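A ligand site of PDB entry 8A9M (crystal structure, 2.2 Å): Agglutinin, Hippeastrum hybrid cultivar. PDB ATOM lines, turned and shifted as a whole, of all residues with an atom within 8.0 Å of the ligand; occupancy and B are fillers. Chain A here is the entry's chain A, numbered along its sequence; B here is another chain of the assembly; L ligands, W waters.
An oxygen (O3) of the ligand sits at hydrogen-bond distance from the side-chain amide oxygen (OE1) of Gln 89 (2.9 Å). O2 of the ligand sits at hydrogen-bond distance from OD2 of Asp 91 (2.7 Å). ND2 of Asn 93 sits at hydrogen-bond distance from O2 of the ligand (3.0 Å). The side-chain hydroxyl (OH) of Tyr 97 lies within hydrogen-bond range of an oxygen (O4) of the ligand (2.8 Å).
N of Gly 105 of chain B sits at hydrogen-bond distance from OD1 of Asn 93 (3.0 Å). The backbone NH (N) of Ala 100 of chain B sits at hydrogen-bond distance from the backbone carbonyl oxygen (O) of Asn 83 of chain B (3.3 Å). The side-chain amide oxygen of Asn 93 sits at hydrogen-bond distance from the backbone NH of Thr 106 of chain B, 3.2 Å away. OH of Tyr 97 is in hydrogen-bond range of NE2 of Gln 89 (2.6 Å). The backbone carbonyl oxygen (O) of Asp 91 is in hydrogen-bond range of the backbone NH (N) of Ile 108 of chain B. OD1 of Asn 93 sits at hydrogen-bond distance from OG1 of Thr 104 of chain B (3.2 Å). The side-chain carboxylate (OD1) of Asp 91 lies within hydrogen-bond range of the backbone NH (N) of Asn 93, 3.1 Å away. The side-chain carboxylate (OD1) of Asp 91 sits close to the side-chain amide oxygen (OE1) of Gln 89 (3.1 Å).
Val 95 touches the ligand. CB of Asn 83 of chain B touches O4 of the ligand, 3.2 Å away. Ala 100 of chain B touches the ligand. Ala 103 of chain B touches the ligand. Asn 107 of chain B touches the ligand (ND2 to O1, 3.8 Å). Hydrophobic or aromatic side chains that line the ligand: Val 95, Tyr 97, Ala 100 of chain B and Ala 103 of chain B. Nine residues have an atom within 4 Å of the ligand: Gln 89, Asp 91, Asn 93, Val 95, Tyr 97, Asn 83 of chain B, Ala 100 of chain B, Ala 103 of chain B and Asn 107 of chain B.
Water W1 lies within hydrogen-bond range of an oxygen (O6) of the ligand (3.1 Å) and the side-chain amide nitrogen (ND2) of Asn 93 (3.3 Å).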
ATOM      1  N   GLN A  89      -7.737   8.087 -14.933  1.00  0.00           N
ATOM      2  CA  GLN A  89      -6.526   8.897 -15.158  1.00  0.00           C
ATOM      3  C   GLN A  89      -5.707   8.291 -16.299  1.00  0.00           C
ATOM      4  O   GLN A  89      -5.865   7.072 -16.576  1.00  0.00           O
ATOM      5  CB  GLN A  89      -5.718   8.979 -13.870  1.00  0.00           C
ATOM      6  CG  GLN A  89      -6.498   9.574 -12.707  1.00  0.00           C
ATOM      7  CD  GLN A  89      -5.609   9.867 -11.518  1.00  0.00           C
ATOM      8  OE1 GLN A  89      -4.505   9.321 -11.366  1.00  0.00           O
ATOM      9  NE2 GLN A  89      -6.070  10.735 -10.666  1.00  0.00           N
ATOM     10  N   LYS A  90      -4.779   9.066 -16.831  1.00  0.00           N
ATOM     11  CA  LYS A  90      -3.815   8.622 -17.874  1.00  0.00           C
ATOM     12  C   LYS A  90      -2.907   7.507 -17.341  1.00  0.00           C
ATOM     13  O   LYS A  90      -2.407   6.731 -18.156  1.00  0.00           O
ATOM     14  CB  LYS A  90      -2.981   9.791 -18.399  1.00  0.00           C
ATOM     15  CG  LYS A  90      -2.238  10.566 -17.346  1.00  0.00           C
ATOM     16  CD  LYS A  90      -1.532  11.757 -17.945  1.00  0.00           C
ATOM     17  CE  LYS A  90      -0.493  12.346 -17.019  1.00  0.00           C
ATOM     18  NZ  LYS A  90      -0.078  13.668 -17.523  1.00  0.00           N
ATOM     19  N   ASP A  91      -2.705   7.434 -16.030  1.00  0.00           N
ATOM     20  CA  ASP A  91      -1.829   6.415 -15.409  1.00  0.00           C
ATOM     21  C   ASP A  91      -2.630   5.140 -15.112  1.00  0.00           C
ATOM     22  O   ASP A  91      -2.062   4.261 -14.490  1.00  0.00           O
ATOM     23  CB  ASP A  91      -1.116   6.984 -14.177  1.00  0.00           C
ATOM     24  CG  ASP A  91      -2.018   7.228 -12.997  1.00  0.00           C
ATOM     25  OD1 ASP A  91      -3.244   7.094 -13.166  1.00  0.00           O
ATOM     26  OD2 ASP A  91      -1.478   7.649 -11.925  1.00  0.00           O
ATOM     27  N   ARG A  92      -3.926   5.086 -15.494  1.00  0.00           N
ATOM     28  CA  ARG A  92      -4.820   3.881 -15.418  1.00  0.00           C
ATOM     29  C   ARG A  92      -5.372   3.690 -13.998  1.00  0.00           C
ATOM     30  O   ARG A  92      -6.142   2.747 -13.776  1.00  0.00           O
ATOM     31  CB  ARG A  92      -4.096   2.616 -15.884  1.00  0.00           C
ATOM     32  CG  ARG A  92      -5.052   1.459 -16.167  1.00  0.00           C
ATOM     33  CD  ARG A  92      -4.317   0.219 -16.586  1.00  0.00           C
ATOM     34  NE  ARG A  92      -3.645  -0.452 -15.487  1.00  0.00           N
ATOM     35  CZ  ARG A  92      -3.017  -1.619 -15.593  1.00  0.00           C
ATOM     36  NH1 ARG A  92      -2.952  -2.239 -16.750  1.00  0.00           N
ATOM     37  NH2 ARG A  92      -2.453  -2.163 -14.521  1.00  0.00           N
ATOM     38  N   ASN A  93      -5.086   4.608 -13.094  1.00  0.00           N
ATOM     39  CA  ASN A  93      -5.766   4.668 -11.778  1.00  0.00           C
ATOM     40  C   ASN A  93      -7.150   5.332 -11.925  1.00  0.00           C
ATOM     41  O   ASN A  93      -7.308   6.279 -12.740  1.00  0.00           O
ATOM     42  CB  ASN A  93      -4.895   5.404 -10.771  1.00  0.00           C
ATOM     43  CG  ASN A  93      -5.049   4.848  -9.383  1.00  0.00           C
ATOM     44  OD1 ASN A  93      -5.753   3.856  -9.175  1.00  0.00           O
ATOM     45  ND2 ASN A  93      -4.397   5.487  -8.422  1.00  0.00           N
ATOM     46  N   VAL A  94      -8.104   4.857 -11.151  1.00  0.00           N
ATOM     47  CA  VAL A  94      -9.433   5.505 -11.003  1.00  0.00           C
ATOM     48  C   VAL A  94      -9.452   6.103  -9.611  1.00  0.00           C
ATOM     49  O   VAL A  94      -9.217   5.352  -8.641  1.00  0.00           O
ATOM     50  CB  VAL A  94     -10.574   4.518 -11.208  1.00  0.00           C
ATOM     51  CG1 VAL A  94     -11.930   5.201 -11.054  1.00  0.00           C
ATOM     52  CG2 VAL A  94     -10.465   3.816 -12.566  1.00  0.00           C
ATOM     53  N   VAL A  95      -9.695   7.416  -9.506  1.00  0.00           N
ATOM     54  CA  VAL A  95      -9.480   8.149  -8.224  1.00  0.00           C
ATOM     55  C   VAL A  95     -10.663   9.082  -7.974  1.00  0.00           C
ATOM     56  O   VAL A  95     -11.105   9.755  -8.912  1.00  0.00           O
ATOM     57  CB  VAL A  95      -8.171   8.955  -8.267  1.00  0.00           C
ATOM     58  CG1 VAL A  95      -7.873   9.619  -6.916  1.00  0.00           C
ATOM     59  CG2 VAL A  95      -7.009   8.109  -8.711  1.00  0.00           C
ATOM     60  N   ILE A  96     -11.089   9.161  -6.722  1.00  0.00           N
ATOM     61  CA  ILE A  96     -12.053  10.203  -6.266  1.00  0.00           C
ATOM     62  C   ILE A  96     -11.265  11.326  -5.604  1.00  0.00           C
ATOM     63  O   ILE A  96     -10.478  11.013  -4.695  1.00  0.00           O
ATOM     64  CB  ILE A  96     -13.121   9.599  -5.322  1.00  0.00           C
ATOM     65  CG1 ILE A  96     -13.926   8.511  -6.039  1.00  0.00           C
ATOM     66  CG2 ILE A  96     -14.021  10.694  -4.742  1.00  0.00           C
ATOM     67  CD1 ILE A  96     -14.830   7.702  -5.149  1.00  0.00           C
ATOM     68  N   TYR A  97     -11.470  12.562  -6.044  1.00  0.00           N
ATOM     69  CA  TYR A  97     -10.864  13.772  -5.454  1.00  0.00           C
ATOM     70  C   TYR A  97     -11.968  14.706  -5.002  1.00  0.00           C
ATOM     71  O   TYR A  97     -12.971  14.874  -5.708  1.00  0.00           O
ATOM     72  CB  TYR A  97     -10.001  14.552  -6.441  1.00  0.00           C
ATOM     73  CG  TYR A  97      -8.774  13.849  -6.974  1.00  0.00           C
ATOM     74  CD1 TYR A  97      -8.854  13.072  -8.120  1.00  0.00           C
ATOM     75  CD2 TYR A  97      -7.528  14.035  -6.408  1.00  0.00           C
ATOM     76  CE1 TYR A  97      -7.728  12.478  -8.668  1.00  0.00           C
ATOM     77  CE2 TYR A  97      -6.403  13.426  -6.924  1.00  0.00           C
ATOM     78  CZ  TYR A  97      -6.503  12.650  -8.070  1.00  0.00           C
ATOM     79  OH  TYR A  97      -5.395  12.080  -8.601  1.00  0.00           O
ATOM     80  N   TYR B   5      -2.133  17.259 -13.091  1.00  0.00           N
ATOM     81  CA  TYR B   5      -1.985  16.473 -11.844  1.00  0.00           C
ATOM     82  C   TYR B   5      -0.945  17.175 -10.974  1.00  0.00           C
ATOM     83  O   TYR B   5       0.019  17.784 -11.504  1.00  0.00           O
ATOM     84  CB  TYR B   5      -1.622  15.016 -12.172  1.00  0.00           C
ATOM     85  CG  TYR B   5      -2.664  14.290 -12.998  1.00  0.00           C
ATOM     86  CD1 TYR B   5      -2.674  14.367 -14.371  1.00  0.00           C
ATOM     87  CD2 TYR B   5      -3.679  13.564 -12.391  1.00  0.00           C
ATOM     88  CE1 TYR B   5      -3.640  13.713 -15.137  1.00  0.00           C
ATOM     89  CE2 TYR B   5      -4.656  12.905 -13.126  1.00  0.00           C
ATOM     90  CZ  TYR B   5      -4.627  12.977 -14.509  1.00  0.00           C
ATOM     91  OH  TYR B   5      -5.593  12.317 -15.243  1.00  0.00           O
ATOM     92  N   SER B   6      -1.089  17.054  -9.655  1.00  0.00           N
ATOM     93  CA  SER B   6      -0.070  17.536  -8.705  1.00  0.00           C
ATOM     94  C   SER B   6       1.270  16.888  -9.065  1.00  0.00           C
ATOM     95  O   SER B   6       1.267  15.705  -9.418  1.00  0.00           O
ATOM     96  CB  SER B   6      -0.495  17.316  -7.261  1.00  0.00           C
ATOM     97  OG  SER B   6      -0.791  15.961  -6.994  1.00  0.00           O
ATOM     98  N   GLY B  82      -0.570  15.861  -0.381  1.00  0.00           N
ATOM     99  CA  GLY B  82      -1.152  14.678  -1.046  1.00  0.00           C
ATOM    100  C   GLY B  82      -1.281  14.883  -2.526  1.00  0.00           C
ATOM    101  O   GLY B  82      -0.449  15.589  -3.110  1.00  0.00           O
ATOM    102  N   ASN B  83      -2.330  14.333  -3.104  1.00  0.00           N
ATOM    103  CA  ASN B  83      -2.583  14.381  -4.553  1.00  0.00           C
ATOM    104  C   ASN B  83      -3.753  15.293  -4.825  1.00  0.00           C
ATOM    105  O   ASN B  83      -4.799  15.118  -4.142  1.00  0.00           O
ATOM    106  CB  ASN B  83      -2.854  12.991  -5.120  1.00  0.00           C
ATOM    107  CG  ASN B  83      -1.650  12.105  -5.013  1.00  0.00           C
ATOM    108  OD1 ASN B  83      -0.661  12.318  -5.681  1.00  0.00           O
ATOM    109  ND2 ASN B  83      -1.738  11.117  -4.141  1.00  0.00           N
ATOM    110  N   TYR B  84      -3.594  16.166  -5.823  1.00  0.00           N
ATOM    111  CA  TYR B  84      -4.606  17.156  -6.227  1.00  0.00           C
ATOM    112  C   TYR B  84      -4.714  17.132  -7.737  1.00  0.00           C
ATOM    113  O   TYR B  84      -3.770  16.632  -8.389  1.00  0.00           O
ATOM    114  CB  TYR B  84      -4.231  18.565  -5.754  1.00  0.00           C
ATOM    115  CG  TYR B  84      -4.237  18.769  -4.258  1.00  0.00           C
ATOM    116  CD1 TYR B  84      -3.151  18.420  -3.487  1.00  0.00           C
ATOM    117  CD2 TYR B  84      -5.325  19.343  -3.606  1.00  0.00           C
ATOM    118  CE1 TYR B  84      -3.135  18.627  -2.112  1.00  0.00           C
ATOM    119  CE2 TYR B  84      -5.340  19.543  -2.230  1.00  0.00           C
ATOM    120  CZ  TYR B  84      -4.233  19.199  -1.480  1.00  0.00           C
ATOM    121  OH  TYR B  84      -4.228  19.394  -0.124  1.00  0.00           O
ATOM    122  N   VAL B  85      -5.783  17.694  -8.275  1.00  0.00           N
ATOM    123  CA  VAL B  85      -5.961  17.906  -9.736  1.00  0.00           C
ATOM    124  C   VAL B  85      -6.494  19.317  -9.927  1.00  0.00           C
ATOM    125  O   VAL B  85      -7.304  19.777  -9.109  1.00  0.00           O
ATOM    126  CB  VAL B  85      -6.902  16.880 -10.391  1.00  0.00           C
ATOM    127  CG1 VAL B  85      -6.259  15.530 -10.562  1.00  0.00           C
ATOM    128  CG2 VAL B  85      -8.207  16.737  -9.641  1.00  0.00           C
ATOM    129  N   THR B  99      -7.991  16.429  -1.212  1.00  0.00           N
ATOM    130  CA  THR B  99      -7.025  15.419  -1.572  1.00  0.00           C
ATOM    131  C   THR B  99      -7.763  14.195  -2.201  1.00  0.00           C
ATOM    132  O   THR B  99      -8.980  14.265  -2.358  1.00  0.00           O
ATOM    133  CB  THR B  99      -6.212  15.216  -0.286  1.00  0.00           C
ATOM    134  OG1 THR B  99      -4.832  15.226  -0.624  1.00  0.00           O
ATOM    135  CG2 THR B  99      -6.571  13.990   0.508  1.00  0.00           C
ATOM    136  N   ALA B 100      -7.028  13.169  -2.618  1.00  0.00           N
ATOM    137  CA  ALA B 100      -7.574  11.867  -3.095  1.00  0.00           C
ATOM    138  C   ALA B 100      -8.221  11.155  -1.916  1.00  0.00           C
ATOM    139  O   ALA B 100      -7.532  10.995  -0.917  1.00  0.00           O
ATOM    140  CB  ALA B 100      -6.481  11.009  -3.668  1.00  0.00           C
ATOM    141  N   ARG B 101      -9.468  10.681  -2.070  1.00  0.00           N
ATOM    142  CA  ARG B 101     -10.250  10.029  -0.989  1.00  0.00           C
ATOM    143  C   ARG B 101     -10.256   8.505  -1.165  1.00  0.00           C
ATOM    144  O   ARG B 101     -10.578   7.815  -0.202  1.00  0.00           O
ATOM    145  CB  ARG B 101     -11.689  10.543  -1.014  1.00  0.00           C
ATOM    146  CG  ARG B 101     -11.809  12.028  -0.682  1.00  0.00           C
ATOM    147  CD  ARG B 101     -11.760  12.280   0.828  1.00  0.00           C
ATOM    148  NE  ARG B 101     -11.874  13.710   1.128  1.00  0.00           N
ATOM    149  CZ  ARG B 101     -10.853  14.574   1.239  1.00  0.00           C
ATOM    150  NH1 ARG B 101     -11.070  15.861   1.468  1.00  0.00           N
ATOM    151  NH2 ARG B 101      -9.605  14.149   1.122  1.00  0.00           N
ATOM    152  N   TRP B 102     -10.047   8.025  -2.392  1.00  0.00           N
ATOM    153  CA  TRP B 102     -10.194   6.588  -2.771  1.00  0.00           C
ATOM    154  C   TRP B 102      -9.598   6.373  -4.167  1.00  0.00           C
ATOM    155  O   TRP B 102      -9.684   7.332  -4.994  1.00  0.00           O
ATOM    156  CB  TRP B 102     -11.668   6.171  -2.730  1.00  0.00           C
ATOM    157  CG  TRP B 102     -11.943   4.752  -3.141  1.00  0.00           C
ATOM    158  CD1 TRP B 102     -11.989   3.663  -2.317  1.00  0.00           C
ATOM    159  CD2 TRP B 102     -12.297   4.261  -4.456  1.00  0.00           C
ATOM    160  NE1 TRP B 102     -12.295   2.540  -3.031  1.00  0.00           N
ATOM    161  CE2 TRP B 102     -12.484   2.875  -4.337  1.00  0.00           C
ATOM    162  CE3 TRP B 102     -12.422   4.861  -5.708  1.00  0.00           C
ATOM    163  CZ2 TRP B 102     -12.788   2.065  -5.427  1.00  0.00           C
ATOM    164  CZ3 TRP B 102     -12.735   4.063  -6.789  1.00  0.00           C
ATOM    165  CH2 TRP B 102     -12.942   2.684  -6.641  1.00  0.00           C
ATOM    166  N   ALA B 103      -9.050   5.185  -4.410  1.00  0.00           N
ATOM    167  CA  ALA B 103      -8.502   4.782  -5.730  1.00  0.00           C
ATOM    168  C   ALA B 103      -8.609   3.263  -5.866  1.00  0.00           C
ATOM    169  O   ALA B 103      -8.659   2.585  -4.855  1.00  0.00           O
ATOM    170  CB  ALA B 103      -7.073   5.247  -5.888  1.00  0.00           C
ATOM    171  N   THR B 104      -8.680   2.795  -7.114  1.00  0.00           N
ATOM    172  CA  THR B 104      -8.635   1.365  -7.464  1.00  0.00           C
ATOM    173  C   THR B 104      -7.230   0.827  -7.193  1.00  0.00           C
ATOM    174  O   THR B 104      -7.119  -0.358  -6.961  1.00  0.00           O
ATOM    175  CB  THR B 104      -9.082   1.167  -8.919  1.00  0.00           C
ATOM    176  OG1 THR B 104      -8.416   2.115  -9.767  1.00  0.00           O
ATOM    177  CG2 THR B 104     -10.574   1.302  -9.084  1.00  0.00           C
ATOM    178  N   GLY B 105      -6.191   1.655  -7.259  1.00  0.00           N
ATOM    179  CA  GLY B 105      -4.797   1.203  -7.111  1.00  0.00           C
ATOM    180  C   GLY B 105      -4.326   0.406  -8.326  1.00  0.00           C
ATOM    181  O   GLY B 105      -3.547  -0.504  -8.154  1.00  0.00           O
ATOM    182  N   THR B 106      -4.750   0.819  -9.521  1.00  0.00           N
ATOM    183  CA  THR B 106      -4.501   0.105 -10.797  1.00  0.00           C
ATOM    184  C   THR B 106      -3.536   0.921 -11.668  1.00  0.00           C
ATOM    185  O   THR B 106      -3.413   0.605 -12.857  1.00  0.00           O
ATOM    186  CB  THR B 106      -5.837  -0.190 -11.479  1.00  0.00           C
ATOM    187  OG1 THR B 106      -6.548   1.039 -11.564  1.00  0.00           O
ATOM    188  CG2 THR B 106      -6.669  -1.206 -10.723  1.00  0.00           C
ATOM    189  N   ASN B 107      -2.859   1.912 -11.079  1.00  0.00           N
ATOM    190  CA  ASN B 107      -1.794   2.739 -11.730  1.00  0.00           C
ATOM    191  C   ASN B 107      -0.698   1.811 -12.293  1.00  0.00           C
ATOM    192  O   ASN B 107      -0.499   0.733 -11.743  1.00  0.00           O
ATOM    193  CB  ASN B 107      -1.215   3.800 -10.766  1.00  0.00           C
ATOM    194  CG  ASN B 107      -0.597   3.206  -9.506  1.00  0.00           C
ATOM    195  OD1 ASN B 107       0.550   2.786  -9.513  1.00  0.00           O
ATOM    196  ND2 ASN B 107      -1.355   3.149  -8.426  1.00  0.00           N
ATOM    197  N   ILE B 108       0.026   2.272 -13.327  1.00  0.00           N
ATOM    198  CA  ILE B 108       1.204   1.582 -13.953  1.00  0.00           C
ATOM    199  C   ILE B 108       2.514   2.230 -13.450  1.00  0.00           C
ATOM    200  O   ILE B 108       2.676   3.472 -13.448  1.00  0.00           O
ATOM    201  CB  ILE B 108       1.111   1.614 -15.491  1.00  0.00           C
ATOM    202  CG1 ILE B 108       0.679   3.002 -16.002  1.00  0.00           C
ATOM    203  CG2 ILE B 108       0.182   0.507 -15.983  1.00  0.00           C
ATOM    204  CD1 ILE B 108       1.082   3.305 -17.447  1.00  0.00           C
HETATM  205  C1  LIG L   1      -1.174   7.724  -7.163  1.00  0.00           C
HETATM  206  C2  LIG L   1      -1.534   8.375  -8.502  1.00  0.00           C
HETATM  207  C3  LIG L   1      -2.272   9.686  -8.153  1.00  0.00           C
HETATM  208  C4  LIG L   1      -3.474   9.373  -7.249  1.00  0.00           C
HETATM  209  C5  LIG L   1      -3.094   8.478  -6.048  1.00  0.00           C
HETATM  210  C6  LIG L   1      -4.329   8.113  -5.248  1.00  0.00           C
HETATM  211  O1  LIG L   1      -0.276   6.640  -7.371  1.00  0.00           O
HETATM  212  O2  LIG L   1      -2.320   7.483  -9.326  1.00  0.00           O
HETATM  213  O3  LIG L   1      -2.678  10.405  -9.320  1.00  0.00           O
HETATM  214  O4  LIG L   1      -4.054  10.559  -6.743  1.00  0.00           O
HETATM  215  O5  LIG L   1      -2.392   7.306  -6.517  1.00  0.00           O
HETATM  216  O6  LIG L   1      -3.984   7.141  -4.269  1.00  0.00           O
HETATM  217  O   HOH W   1      -3.740   4.291  -5.456  1.00  0.00           O
